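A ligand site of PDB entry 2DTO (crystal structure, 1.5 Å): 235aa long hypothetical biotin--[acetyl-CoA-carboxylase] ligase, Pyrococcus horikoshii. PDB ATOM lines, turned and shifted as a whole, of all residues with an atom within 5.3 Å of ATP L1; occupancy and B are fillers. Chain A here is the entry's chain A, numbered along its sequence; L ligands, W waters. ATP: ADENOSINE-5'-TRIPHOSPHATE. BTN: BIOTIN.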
ATOM      1  N   GLY A  47      22.178  19.501 -15.359  1.00  0.00           N
ATOM      2  CA  GLY A  47      20.865  19.514 -15.963  1.00  0.00           C
ATOM      3  C   GLY A  47      20.500  18.046 -16.040  1.00  0.00           C
ATOM      4  O   GLY A  47      20.877  17.279 -15.148  1.00  0.00           O
ATOM      5  N   ARG A  48      19.793  17.624 -17.083  1.00  0.00           N
ATOM      6  CA  ARG A  48      19.442  16.216 -17.214  1.00  0.00           C
ATOM      7  C   ARG A  48      20.669  15.404 -17.624  1.00  0.00           C
ATOM      8  O   ARG A  48      21.657  15.968 -18.104  1.00  0.00           O
ATOM      9  CB  ARG A  48      18.366  16.002 -18.290  1.00  0.00           C
ATOM     10  CG  ARG A  48      17.058  16.720 -18.060  1.00  0.00           C
ATOM     11  CD  ARG A  48      16.166  16.511 -19.276  1.00  0.00           C
ATOM     12  NE  ARG A  48      16.807  17.025 -20.492  1.00  0.00           N
ATOM     13  CZ  ARG A  48      16.415  16.734 -21.727  1.00  0.00           C
ATOM     14  NH1 ARG A  48      15.378  15.933 -21.932  1.00  0.00           N
ATOM     15  NH2 ARG A  48      17.069  17.259 -22.760  1.00  0.00           N
ATOM     16  N   ARG A  51      24.399  16.469 -17.381  1.00  0.00           N
ATOM     17  CA  ARG A  51      25.007  17.474 -18.248  1.00  0.00           C
ATOM     18  C   ARG A  51      25.425  18.641 -17.370  1.00  0.00           C
ATOM     19  O   ARG A  51      24.680  19.076 -16.495  1.00  0.00           O
ATOM     20  CB  ARG A  51      24.013  17.924 -19.310  1.00  0.00           C
ATOM     21  CG  ARG A  51      23.680  16.818 -20.299  1.00  0.00           C
ATOM     22  CD  ARG A  51      22.496  17.164 -21.192  1.00  0.00           C
ATOM     23  NE  ARG A  51      22.257  16.104 -22.159  1.00  0.00           N
ATOM     24  CZ  ARG A  51      21.159  15.994 -22.912  1.00  0.00           C
ATOM     25  NH1 ARG A  51      20.195  16.894 -22.804  1.00  0.00           N
ATOM     26  NH2 ARG A  51      21.034  14.981 -23.762  1.00  0.00           N
ATOM     27  N   LYS A  52      26.631  19.151 -17.595  1.00  0.00           N
ATOM     28  CA  LYS A  52      27.139  20.242 -16.783  1.00  0.00           C
ATOM     29  C   LYS A  52      26.354  21.549 -16.915  1.00  0.00           C
ATOM     30  O   LYS A  52      26.049  21.994 -18.027  1.00  0.00           O
ATOM     31  CB  LYS A  52      28.610  20.511 -17.113  1.00  0.00           C
ATOM     32  CG  LYS A  52      29.234  21.703 -16.378  1.00  0.00           C
ATOM     33  CD  LYS A  52      29.504  21.367 -14.927  1.00  0.00           C
ATOM     34  CE  LYS A  52      30.628  22.223 -14.334  1.00  0.00           C
ATOM     35  NZ  LYS A  52      31.046  21.742 -12.988  1.00  0.00           N
ATOM     36  N   TRP A  53      26.025  22.145 -15.780  1.00  0.00           N
ATOM     37  CA  TRP A  53      25.341  23.427 -15.760  1.00  0.00           C
ATOM     38  C   TRP A  53      26.306  24.419 -15.139  1.00  0.00           C
ATOM     39  O   TRP A  53      26.655  24.310 -13.965  1.00  0.00           O
ATOM     40  CB  TRP A  53      24.057  23.359 -14.926  1.00  0.00           C
ATOM     41  CG  TRP A  53      23.346  24.687 -14.830  1.00  0.00           C
ATOM     42  CD1 TRP A  53      23.481  25.620 -13.828  1.00  0.00           C
ATOM     43  CD2 TRP A  53      22.475  25.264 -15.800  1.00  0.00           C
ATOM     44  NE1 TRP A  53      22.735  26.744 -14.135  1.00  0.00           N
ATOM     45  CE2 TRP A  53      22.117  26.549 -15.338  1.00  0.00           C
ATOM     46  CE3 TRP A  53      21.969  24.827 -17.035  1.00  0.00           C
ATOM     47  CZ2 TRP A  53      21.261  27.402 -16.059  1.00  0.00           C
ATOM     48  CZ3 TRP A  53      21.119  25.665 -17.744  1.00  0.00           C
ATOM     49  CH2 TRP A  53      20.778  26.941 -17.253  1.00  0.00           C
ATOM     50  N   GLU A  54      26.759  25.382 -15.952  1.00  0.00           N
ATOM     51  CA  GLU A  54      27.693  26.405 -15.483  1.00  0.00           C
ATOM     52  C   GLU A  54      27.007  27.276 -14.441  1.00  0.00           C
ATOM     53  O   GLU A  54      25.993  27.910 -14.741  1.00  0.00           O
ATOM     54  CB  GLU A  54      28.159  27.261 -16.655  1.00  0.00           C
ATOM     55  CG  GLU A  54      28.862  26.492 -17.766  1.00  0.00           C
ATOM     56  CD  GLU A  54      30.105  25.772 -17.294  1.00  0.00           C
ATOM     57  OE1 GLU A  54      30.848  26.354 -16.466  1.00  0.00           O
ATOM     58  OE2 GLU A  54      30.355  24.637 -17.740  1.00  0.00           O
ATOM     59  N   SER A  55      27.567  27.323 -13.239  1.00  0.00           N
ATOM     60  CA  SER A  55      26.963  28.076 -12.138  1.00  0.00           C
ATOM     61  C   SER A  55      27.924  29.028 -11.444  1.00  0.00           C
ATOM     62  O   SER A  55      28.202  28.885 -10.254  1.00  0.00           O
ATOM     63  CB  SER A  55      26.412  27.095 -11.114  1.00  0.00           C
ATOM     64  OG  SER A  55      25.712  26.034 -11.738  1.00  0.00           O
ATOM     65  N   TRP A  61      20.977  30.279  -8.487  1.00  0.00           N
ATOM     66  CA  TRP A  61      20.966  28.822  -8.532  1.00  0.00           C
ATOM     67  C   TRP A  61      20.217  28.324  -7.302  1.00  0.00           C
ATOM     68  O   TRP A  61      20.688  28.462  -6.173  1.00  0.00           O
ATOM     69  CB  TRP A  61      22.418  28.307  -8.512  1.00  0.00           C
ATOM     70  CG  TRP A  61      23.406  29.171  -9.283  1.00  0.00           C
ATOM     71  CD1 TRP A  61      24.535  29.770  -8.785  1.00  0.00           C
ATOM     72  CD2 TRP A  61      23.337  29.555 -10.668  1.00  0.00           C
ATOM     73  NE1 TRP A  61      25.173  30.490  -9.763  1.00  0.00           N
ATOM     74  CE2 TRP A  61      24.460  30.373 -10.930  1.00  0.00           C
ATOM     75  CE3 TRP A  61      22.436  29.279 -11.703  1.00  0.00           C
ATOM     76  CZ2 TRP A  61      24.704  30.927 -12.190  1.00  0.00           C
ATOM     77  CZ3 TRP A  61      22.688  29.833 -12.968  1.00  0.00           C
ATOM     78  CH2 TRP A  61      23.812  30.642 -13.190  1.00  0.00           C
ATOM     79  N   LYS A 100      10.623  27.687 -23.867  1.00  0.00           N
ATOM     80  CA  LYS A 100      11.012  26.714 -24.866  1.00  0.00           C
ATOM     81  C   LYS A 100      10.594  25.436 -24.136  1.00  0.00           C
ATOM     82  O   LYS A 100      11.218  25.041 -23.150  1.00  0.00           O
ATOM     83  CB  LYS A 100      12.528  26.728 -25.084  1.00  0.00           C
ATOM     84  CG  LYS A 100      13.047  25.551 -25.903  1.00  0.00           C
ATOM     85  CD  LYS A 100      14.542  25.703 -26.174  1.00  0.00           C
ATOM     86  CE  LYS A 100      15.107  24.499 -26.914  1.00  0.00           C
ATOM     87  NZ  LYS A 100      15.241  23.293 -26.051  1.00  0.00           N
ATOM     88  N   ASN A 103      11.066  22.980 -20.309  1.00  0.00           N
ATOM     89  CA  ASN A 103      11.936  23.387 -19.205  1.00  0.00           C
ATOM     90  C   ASN A 103      12.885  24.566 -19.382  1.00  0.00           C
ATOM     91  O   ASN A 103      13.641  24.880 -18.456  1.00  0.00           O
ATOM     92  CB  ASN A 103      12.766  22.178 -18.814  1.00  0.00           C
ATOM     93  CG  ASN A 103      13.725  21.758 -19.918  1.00  0.00           C
ATOM     94  OD1 ASN A 103      13.487  22.063 -21.095  1.00  0.00           O
ATOM     95  ND2 ASN A 103      14.798  21.076 -19.558  1.00  0.00           N
ATOM     96  N   ASP A 104      12.864  25.212 -20.539  1.00  0.00           N
ATOM     97  CA  ASP A 104      13.780  26.317 -20.775  1.00  0.00           C
ATOM     98  C   ASP A 104      13.102  27.656 -21.001  1.00  0.00           C
ATOM     99  O   ASP A 104      11.959  27.728 -21.453  1.00  0.00           O
ATOM    100  CB  ASP A 104      14.669  26.004 -21.996  1.00  0.00           C
ATOM    101  CG  ASP A 104      15.501  24.751 -21.822  1.00  0.00           C
ATOM    102  OD1 ASP A 104      16.018  24.515 -20.720  1.00  0.00           O
ATOM    103  OD2 ASP A 104      15.662  24.002 -22.811  1.00  0.00           O
ATOM    104  N   LYS A 111      19.184  31.004 -24.390  1.00  0.00           N
ATOM    105  CA  LYS A 111      18.797  30.451 -23.096  1.00  0.00           C
ATOM    106  C   LYS A 111      19.241  31.295 -21.902  1.00  0.00           C
ATOM    107  O   LYS A 111      20.431  31.548 -21.702  1.00  0.00           O
ATOM    108  CB  LYS A 111      19.331  29.030 -22.980  1.00  0.00           C
ATOM    109  CG  LYS A 111      18.857  28.277 -21.739  1.00  0.00           C
ATOM    110  CD  LYS A 111      19.211  26.810 -21.874  1.00  0.00           C
ATOM    111  CE  LYS A 111      18.771  26.015 -20.656  1.00  0.00           C
ATOM    112  NZ  LYS A 111      19.140  24.585 -20.822  1.00  0.00           N
ATOM    113  N   LEU A 116      14.935  21.998 -13.801  1.00  0.00           N
ATOM    114  CA  LEU A 116      15.172  20.569 -13.677  1.00  0.00           C
ATOM    115  C   LEU A 116      14.418  20.030 -12.479  1.00  0.00           C
ATOM    116  O   LEU A 116      14.703  20.420 -11.347  1.00  0.00           O
ATOM    117  CB  LEU A 116      16.664  20.270 -13.486  1.00  0.00           C
ATOM    118  CG  LEU A 116      17.003  18.784 -13.269  1.00  0.00           C
ATOM    119  CD1 LEU A 116      16.655  17.983 -14.515  1.00  0.00           C
ATOM    120  CD2 LEU A 116      18.479  18.633 -12.943  1.00  0.00           C
ATOM    121  N   ASN A 131      20.426  32.881 -15.268  1.00  0.00           N
ATOM    122  CA  ASN A 131      21.595  33.728 -15.432  1.00  0.00           C
ATOM    123  C   ASN A 131      21.196  35.174 -15.157  1.00  0.00           C
ATOM    124  O   ASN A 131      20.318  35.726 -15.821  1.00  0.00           O
ATOM    125  CB  ASN A 131      22.171  33.618 -16.850  1.00  0.00           C
ATOM    126  CG  ASN A 131      22.634  32.217 -17.192  1.00  0.00           C
ATOM    127  OD1 ASN A 131      23.393  31.599 -16.455  1.00  0.00           O
ATOM    128  ND2 ASN A 131      22.183  31.703 -18.334  1.00  0.00           N
ATOM    129  N   ASN A 134      26.003  36.862 -13.948  1.00  0.00           N
ATOM    130  CA  ASN A 134      27.129  35.976 -14.256  1.00  0.00           C
ATOM    131  C   ASN A 134      27.497  35.873 -15.732  1.00  0.00           C
ATOM    132  O   ASN A 134      26.684  36.174 -16.607  1.00  0.00           O
ATOM    133  CB  ASN A 134      26.814  34.560 -13.769  1.00  0.00           C
ATOM    134  CG  ASN A 134      25.515  34.027 -14.360  1.00  0.00           C
ATOM    135  OD1 ASN A 134      24.443  34.515 -14.045  1.00  0.00           O
ATOM    136  ND2 ASN A 134      25.630  33.025 -15.234  1.00  0.00           N
ATOM    137  N   VAL A 136      28.108  33.835 -19.050  1.00  0.00           N
ATOM    138  CA  VAL A 136      27.379  32.682 -19.549  1.00  0.00           C
ATOM    139  C   VAL A 136      28.064  32.025 -20.748  1.00  0.00           C
ATOM    140  O   VAL A 136      28.901  32.653 -21.406  1.00  0.00           O
ATOM    141  CB  VAL A 136      25.957  33.086 -19.996  1.00  0.00           C
ATOM    142  CG1 VAL A 136      25.210  33.732 -18.843  1.00  0.00           C
ATOM    143  CG2 VAL A 136      26.021  34.043 -21.181  1.00  0.00           C
ATOM    144  N   PRO A 137      27.742  30.759 -21.025  1.00  0.00           N
ATOM    145  CA  PRO A 137      28.350  30.037 -22.160  1.00  0.00           C
ATOM    146  C   PRO A 137      27.690  30.493 -23.465  1.00  0.00           C
ATOM    147  O   PRO A 137      26.665  31.180 -23.443  1.00  0.00           O
ATOM    148  CB  PRO A 137      28.053  28.580 -21.841  1.00  0.00           C
ATOM    149  CG  PRO A 137      26.748  28.646 -21.100  1.00  0.00           C
ATOM    150  CD  PRO A 137      26.955  29.837 -20.187  1.00  0.00           C
ATOM    151  N   ALA A 140      23.754  31.177 -24.747  1.00  0.00           N
ATOM    152  CA  ALA A 140      23.022  31.660 -23.590  1.00  0.00           C
ATOM    153  C   ALA A 140      23.071  33.173 -23.440  1.00  0.00           C
ATOM    154  O   ALA A 140      23.815  33.876 -24.137  1.00  0.00           O
ATOM    155  CB  ALA A 140      23.567  31.010 -22.329  1.00  0.00           C
ATOM    156  N   TYR A 227       8.417  15.045 -22.911  1.00  0.00           N
ATOM    157  CA  TYR A 227       9.823  15.440 -22.933  1.00  0.00           C
ATOM    158  C   TYR A 227      10.825  14.343 -22.584  1.00  0.00           C
ATOM    159  O   TYR A 227      11.673  13.987 -23.399  1.00  0.00           O
ATOM    160  CB  TYR A 227      10.057  16.660 -22.034  1.00  0.00           C
ATOM    161  CG  TYR A 227      11.326  17.423 -22.385  1.00  0.00           C
ATOM    162  CD1 TYR A 227      11.542  17.860 -23.695  1.00  0.00           C
ATOM    163  CD2 TYR A 227      12.290  17.716 -21.419  1.00  0.00           C
ATOM    164  CE1 TYR A 227      12.693  18.568 -24.030  1.00  0.00           C
ATOM    165  CE2 TYR A 227      13.446  18.431 -21.748  1.00  0.00           C
ATOM    166  CZ  TYR A 227      13.637  18.854 -23.060  1.00  0.00           C
ATOM    167  OH  TYR A 227      14.775  19.555 -23.380  1.00  0.00           O
ATOM    168  N   SER A 231      15.452  16.019 -26.790  1.00  0.00           N
ATOM    169  CA  SER A 231      15.873  17.402 -26.858  1.00  0.00           C
ATOM    170  C   SER A 231      15.078  18.063 -27.973  1.00  0.00           C
ATOM    171  O   SER A 231      14.725  17.425 -28.967  1.00  0.00           O
ATOM    172  CB  SER A 231      17.369  17.512 -27.149  1.00  0.00           C
ATOM    173  OG  SER A 231      18.124  17.267 -25.975  1.00  0.00           O
ATOM    174  N   LEU A 232      14.781  19.341 -27.785  1.00  0.00           N
ATOM    175  CA  LEU A 232      14.026  20.108 -28.768  1.00  0.00           C
ATOM    176  C   LEU A 232      14.942  21.168 -29.344  1.00  0.00           C
ATOM    177  O   LEU A 232      15.627  21.877 -28.612  1.00  0.00           O
ATOM    178  CB  LEU A 232      12.804  20.749 -28.093  1.00  0.00           C
ATOM    179  CG  LEU A 232      11.830  21.576 -28.936  1.00  0.00           C
ATOM    180  CD1 LEU A 232      10.541  21.766 -28.147  1.00  0.00           C
ATOM    181  CD2 LEU A 232      12.443  22.921 -29.291  1.00  0.00           C
ATOM    182  N   ARG A 233      14.945  21.270 -30.667  1.00  0.00           N
ATOM    183  CA  ARG A 233      15.763  22.241 -31.372  1.00  0.00           C
ATOM    184  C   ARG A 233      14.929  23.084 -32.312  1.00  0.00           C
ATOM    185  O   ARG A 233      14.004  22.588 -32.955  1.00  0.00           O
ATOM    186  CB  ARG A 233      16.851  21.518 -32.180  1.00  0.00           C
ATOM    187  CG  ARG A 233      17.881  20.796 -31.338  1.00  0.00           C
ATOM    188  CD  ARG A 233      18.866  21.767 -30.722  1.00  0.00           C
ATOM    189  NE  ARG A 233      19.816  21.094 -29.838  1.00  0.00           N
ATOM    190  CZ  ARG A 233      19.541  20.732 -28.587  1.00  0.00           C
ATOM    191  NH1 ARG A 233      18.351  20.992 -28.064  1.00  0.00           N
ATOM    192  NH2 ARG A 233      20.457  20.112 -27.860  1.00  0.00           N
HETATM  193  PG  ATP L   1      19.466  20.607 -24.427  1.00  0.00           P
HETATM  194  O1G ATP L   1      20.729  21.388 -24.192  1.00  0.00           O
HETATM  195  O2G ATP L   1      19.806  19.309 -25.158  1.00  0.00           O
HETATM  196  O3G ATP L   1      18.504  21.441 -25.269  1.00  0.00           O
HETATM  197  PB  ATP L   1      17.948  21.026 -21.939  1.00  0.00           P
HETATM  198  O1B ATP L   1      16.619  20.421 -21.608  1.00  0.00           O
HETATM  199  O2B ATP L   1      17.757  22.413 -22.462  1.00  0.00           O
HETATM  200  O3B ATP L   1      18.768  20.098 -23.031  1.00  0.00           O
HETATM  201  PA  ATP L   1      19.609  19.842 -19.923  1.00  0.00           P
HETATM  202  O1A ATP L   1      18.862  19.465 -18.709  1.00  0.00           O
HETATM  203  O2A ATP L   1      19.690  18.673 -20.838  1.00  0.00           O
HETATM  204  O3A ATP L   1      18.944  21.125 -20.684  1.00  0.00           O
HETATM  205  O5' ATP L   1      21.041  20.355 -19.402  1.00  0.00           O
HETATM  206  C5' ATP L   1      21.560  21.726 -19.560  1.00  0.00           C
HETATM  207  C4' ATP L   1      22.249  22.193 -20.832  1.00  0.00           C
HETATM  208  O4' ATP L   1      22.268  23.667 -20.734  1.00  0.00           O
HETATM  209  C3' ATP L   1      23.710  21.795 -21.014  1.00  0.00           C
HETATM  210  O3' ATP L   1      23.818  20.612 -21.823  1.00  0.00           O
HETATM  211  C2' ATP L   1      24.347  23.053 -21.586  1.00  0.00           C
HETATM  212  O2' ATP L   1      24.463  23.017 -23.018  1.00  0.00           O
HETATM  213  C1' ATP L   1      23.488  24.233 -21.193  1.00  0.00           C
HETATM  214  N9  ATP L   1      23.970  25.131 -20.091  1.00  0.00           N
HETATM  215  C8  ATP L   1      24.889  24.896 -19.053  1.00  0.00           C
HETATM  216  N7  ATP L   1      25.081  25.931 -18.249  1.00  0.00           N
HETATM  217  C5  ATP L   1      24.245  26.906 -18.752  1.00  0.00           C
HETATM  218  C6  ATP L   1      23.960  28.263 -18.344  1.00  0.00           C
HETATM  219  N6  ATP L   1      24.539  28.857 -17.280  1.00  0.00           N
HETATM  220  N1  ATP L   1      23.034  29.014 -19.106  1.00  0.00           N
HETATM  221  C2  ATP L   1      22.437  28.430 -20.200  1.00  0.00           C
HETATM  222  N3  ATP L   1      22.632  27.162 -20.663  1.00  0.00           N
HETATM  223  C4  ATP L   1      23.550  26.440 -19.895  1.00  0.00           C
HETATM  224  C11 BTN L   2      17.970  22.856 -17.816  1.00  0.00           C
HETATM  225  O11 BTN L   2      16.791  22.802 -18.272  1.00  0.00           O
HETATM  226  O12 BTN L   2      18.936  23.285 -18.514  1.00  0.00           O
HETATM  227  C10 BTN L   2      18.307  22.423 -16.410  1.00  0.00           C
HETATM  228  C9  BTN L   2      19.225  23.212 -15.555  1.00  0.00           C
HETATM  229  C8  BTN L   2      18.874  23.245 -14.110  1.00  0.00           C
HETATM  230  C7  BTN L   2      19.859  24.093 -13.338  1.00  0.00           C
HETATM  231  C2  BTN L   2      19.621  24.248 -11.836  1.00  0.00           C
HETATM  232  S1  BTN L   2      20.843  25.282 -11.050  1.00  0.00           S
HETATM  233  C6  BTN L   2      19.985  24.945  -9.490  1.00  0.00           C
HETATM  234  C5  BTN L   2      19.856  23.392  -9.539  1.00  0.00           C
HETATM  235  N1  BTN L   2      21.094  22.702  -9.095  1.00  0.00           N
HETATM  236  C3  BTN L   2      21.572  21.913 -10.117  1.00  0.00           C
HETATM  237  O3  BTN L   2      22.599  21.207 -10.075  1.00  0.00           O
HETATM  238  N2  BTN L   2      20.750  22.014 -11.229  1.00  0.00           N
HETATM  239  C4  BTN L   2      19.633  22.911 -10.984  1.00  0.00           C
HETATM  240  O   HOH W   1      27.228  20.756 -21.071  1.00  0.00           O
HETATM  241  O   HOH W   2      16.222  19.726 -17.513  1.00  0.00           O
HETATM  242  O   HOH W   3      17.812  23.909 -25.301  1.00  0.00           O
HETATM  243  O   HOH W   4      24.751  18.689 -23.394  1.00  0.00           O
HETATM  244  O   HOH W   5      15.966  20.453 -25.472  1.00  0.00           O
HETATM  245  O   HOH W   6      25.519  25.916 -23.597  1.00  0.00           O
HETATM  246  O   HOH W   7      20.781  24.207 -23.576  1.00  0.00           O
HETATM  247  O   HOH W   8      22.907  27.394 -23.784  1.00  0.00           O
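NE of Arg 48 lies within salt-bridge range of O2A of ATP L1, 3.3 Å away. A nitrogen (N1) of ATP L1 is in hydrogen-bond range of the side-chain amide nitrogen (ND2) of Asn 131 (2.9 Å). The side-chain hydroxyl (OG) of Ser 231 lies within hydrogen-bond range of an oxygen (O2G) of ATP L1 (2.8 Å). O2B of ATP L1 sits close to OD2 of Asp 104 (2.7 Å). O3G of ATP L1 lies within salt-bridge range of NH1 of Arg 233 (2.8 Å). N7 of ATP L1 is in hydrogen-bond range of N of Glu 54, 2.9 Å away. O2A of ATP L1 lies within salt-bridge range of NH1 of Arg 51 (2.7 Å). NZ of Lys 100 lies within salt-bridge range of O3G of ATP L1. An oxygen (O12) of BTN L2 is in salt-bridge range of the side-chain amino group (NZ) of Lys 111 (2.7 Å). NZ of Lys 111 is in salt-bridge range of O2B of ATP L1, at 3.1 Å. The backbone carbonyl oxygen of Glu 54 sits at hydrogen-bond distance from a nitrogen (N6) of ATP L1 (3.1 Å). The side-chain hydroxyl (OH) of Tyr 227 sits at hydrogen-bond distance from an oxygen (O1B) of ATP L1 (2.7 Å). An oxygen (O1A) of ATP L1 is in hydrogen-bond range of the backbone NH (N) of Arg 48 (2.6 Å). ND2 of Asn 103 sits at hydrogen-bond distance from O1B of ATP L1. ND2 of Asn 103 sits at hydrogen-bond distance from O11 of BTN L2. OD1 of Asp 104 sits close to O11 of BTN L2, at 3.1 Å.
The backbone carbonyl oxygen of Trp 53 sits at hydrogen-bond distance from the side-chain hydroxyl of Ser 55. The side-chain amino group (NZ) of Lys 100 sits at hydrogen-bond distance from the backbone carbonyl oxygen (O) of Leu 232 (3.0 Å). The side-chain hydroxyl (OG) of Ser 231 lies within hydrogen-bond range of the guanidinium group (NH2) of Arg 48, at 3.4 Å. OD2 of Asp 104 sits close to OD1 of Asn 103 (3.4 Å). The guanidinium group (NH2) of Arg 48 lies within hydrogen-bond range of the side-chain hydroxyl (OH) of Tyr 227 (3.3 Å). The side-chain carboxylate (OD1) of Asp 104 is in salt-bridge range of the side-chain amino group (NZ) of Lys 111. The side-chain amide nitrogen of Asn 134 sits at hydrogen-bond distance from the side-chain amide oxygen of Asn 131, at 2.9 Å. OD2 of Asp 104 is in salt-bridge range of NZ of Lys 100.
CA of Gly 47 touches O1A of ATP L1, 3.4 Å away. Lys 52 touches ATP L1. Trp 53 touches ATP L1. Pro 137 touches ATP L1. CB of Ala 140 touches C2 of ATP L1 (3.5 Å). 16 residues have an atom within 4 Å of ATP L1: Gly 47, Arg 48, Arg 51, Lys 52, Trp 53, Glu 54, Lys 100, Asn 103, Asp 104, Lys 111, Asn 131, Pro 137, Ala 140, Tyr 227, Ser 231 and Arg 233.
Water W3 lies within hydrogen-bond range of an oxygen (O3G) of ATP L1 (2.6 Å), the side-chain amino group of Lys 100 (2.7 Å) and the side-chain carboxylate of Asp 104 (3.3 Å). Water W5 lies within hydrogen-bond range of OH of Tyr 227, O3G of ATP L1, N of Leu 232 and NZ of Lys 100. Water W7 lies within hydrogen-bond range of O1G of ATP L1 and NZ of Lys 111. Water W2 lies within hydrogen-bond range of ND2 of Asn 103 (2.8 Å), O1A of ATP L1 (2.9 Å) and O11 of BTN L2 (3.2 Å). Water W1 bridges O of Lys 52 (3.5 Å) and O3' of ATP L1 (3.5 Å).
An oxygen (O3A) of ATP L1 sits close to an oxygen (O12) of BTN L2 (3.1 Å).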
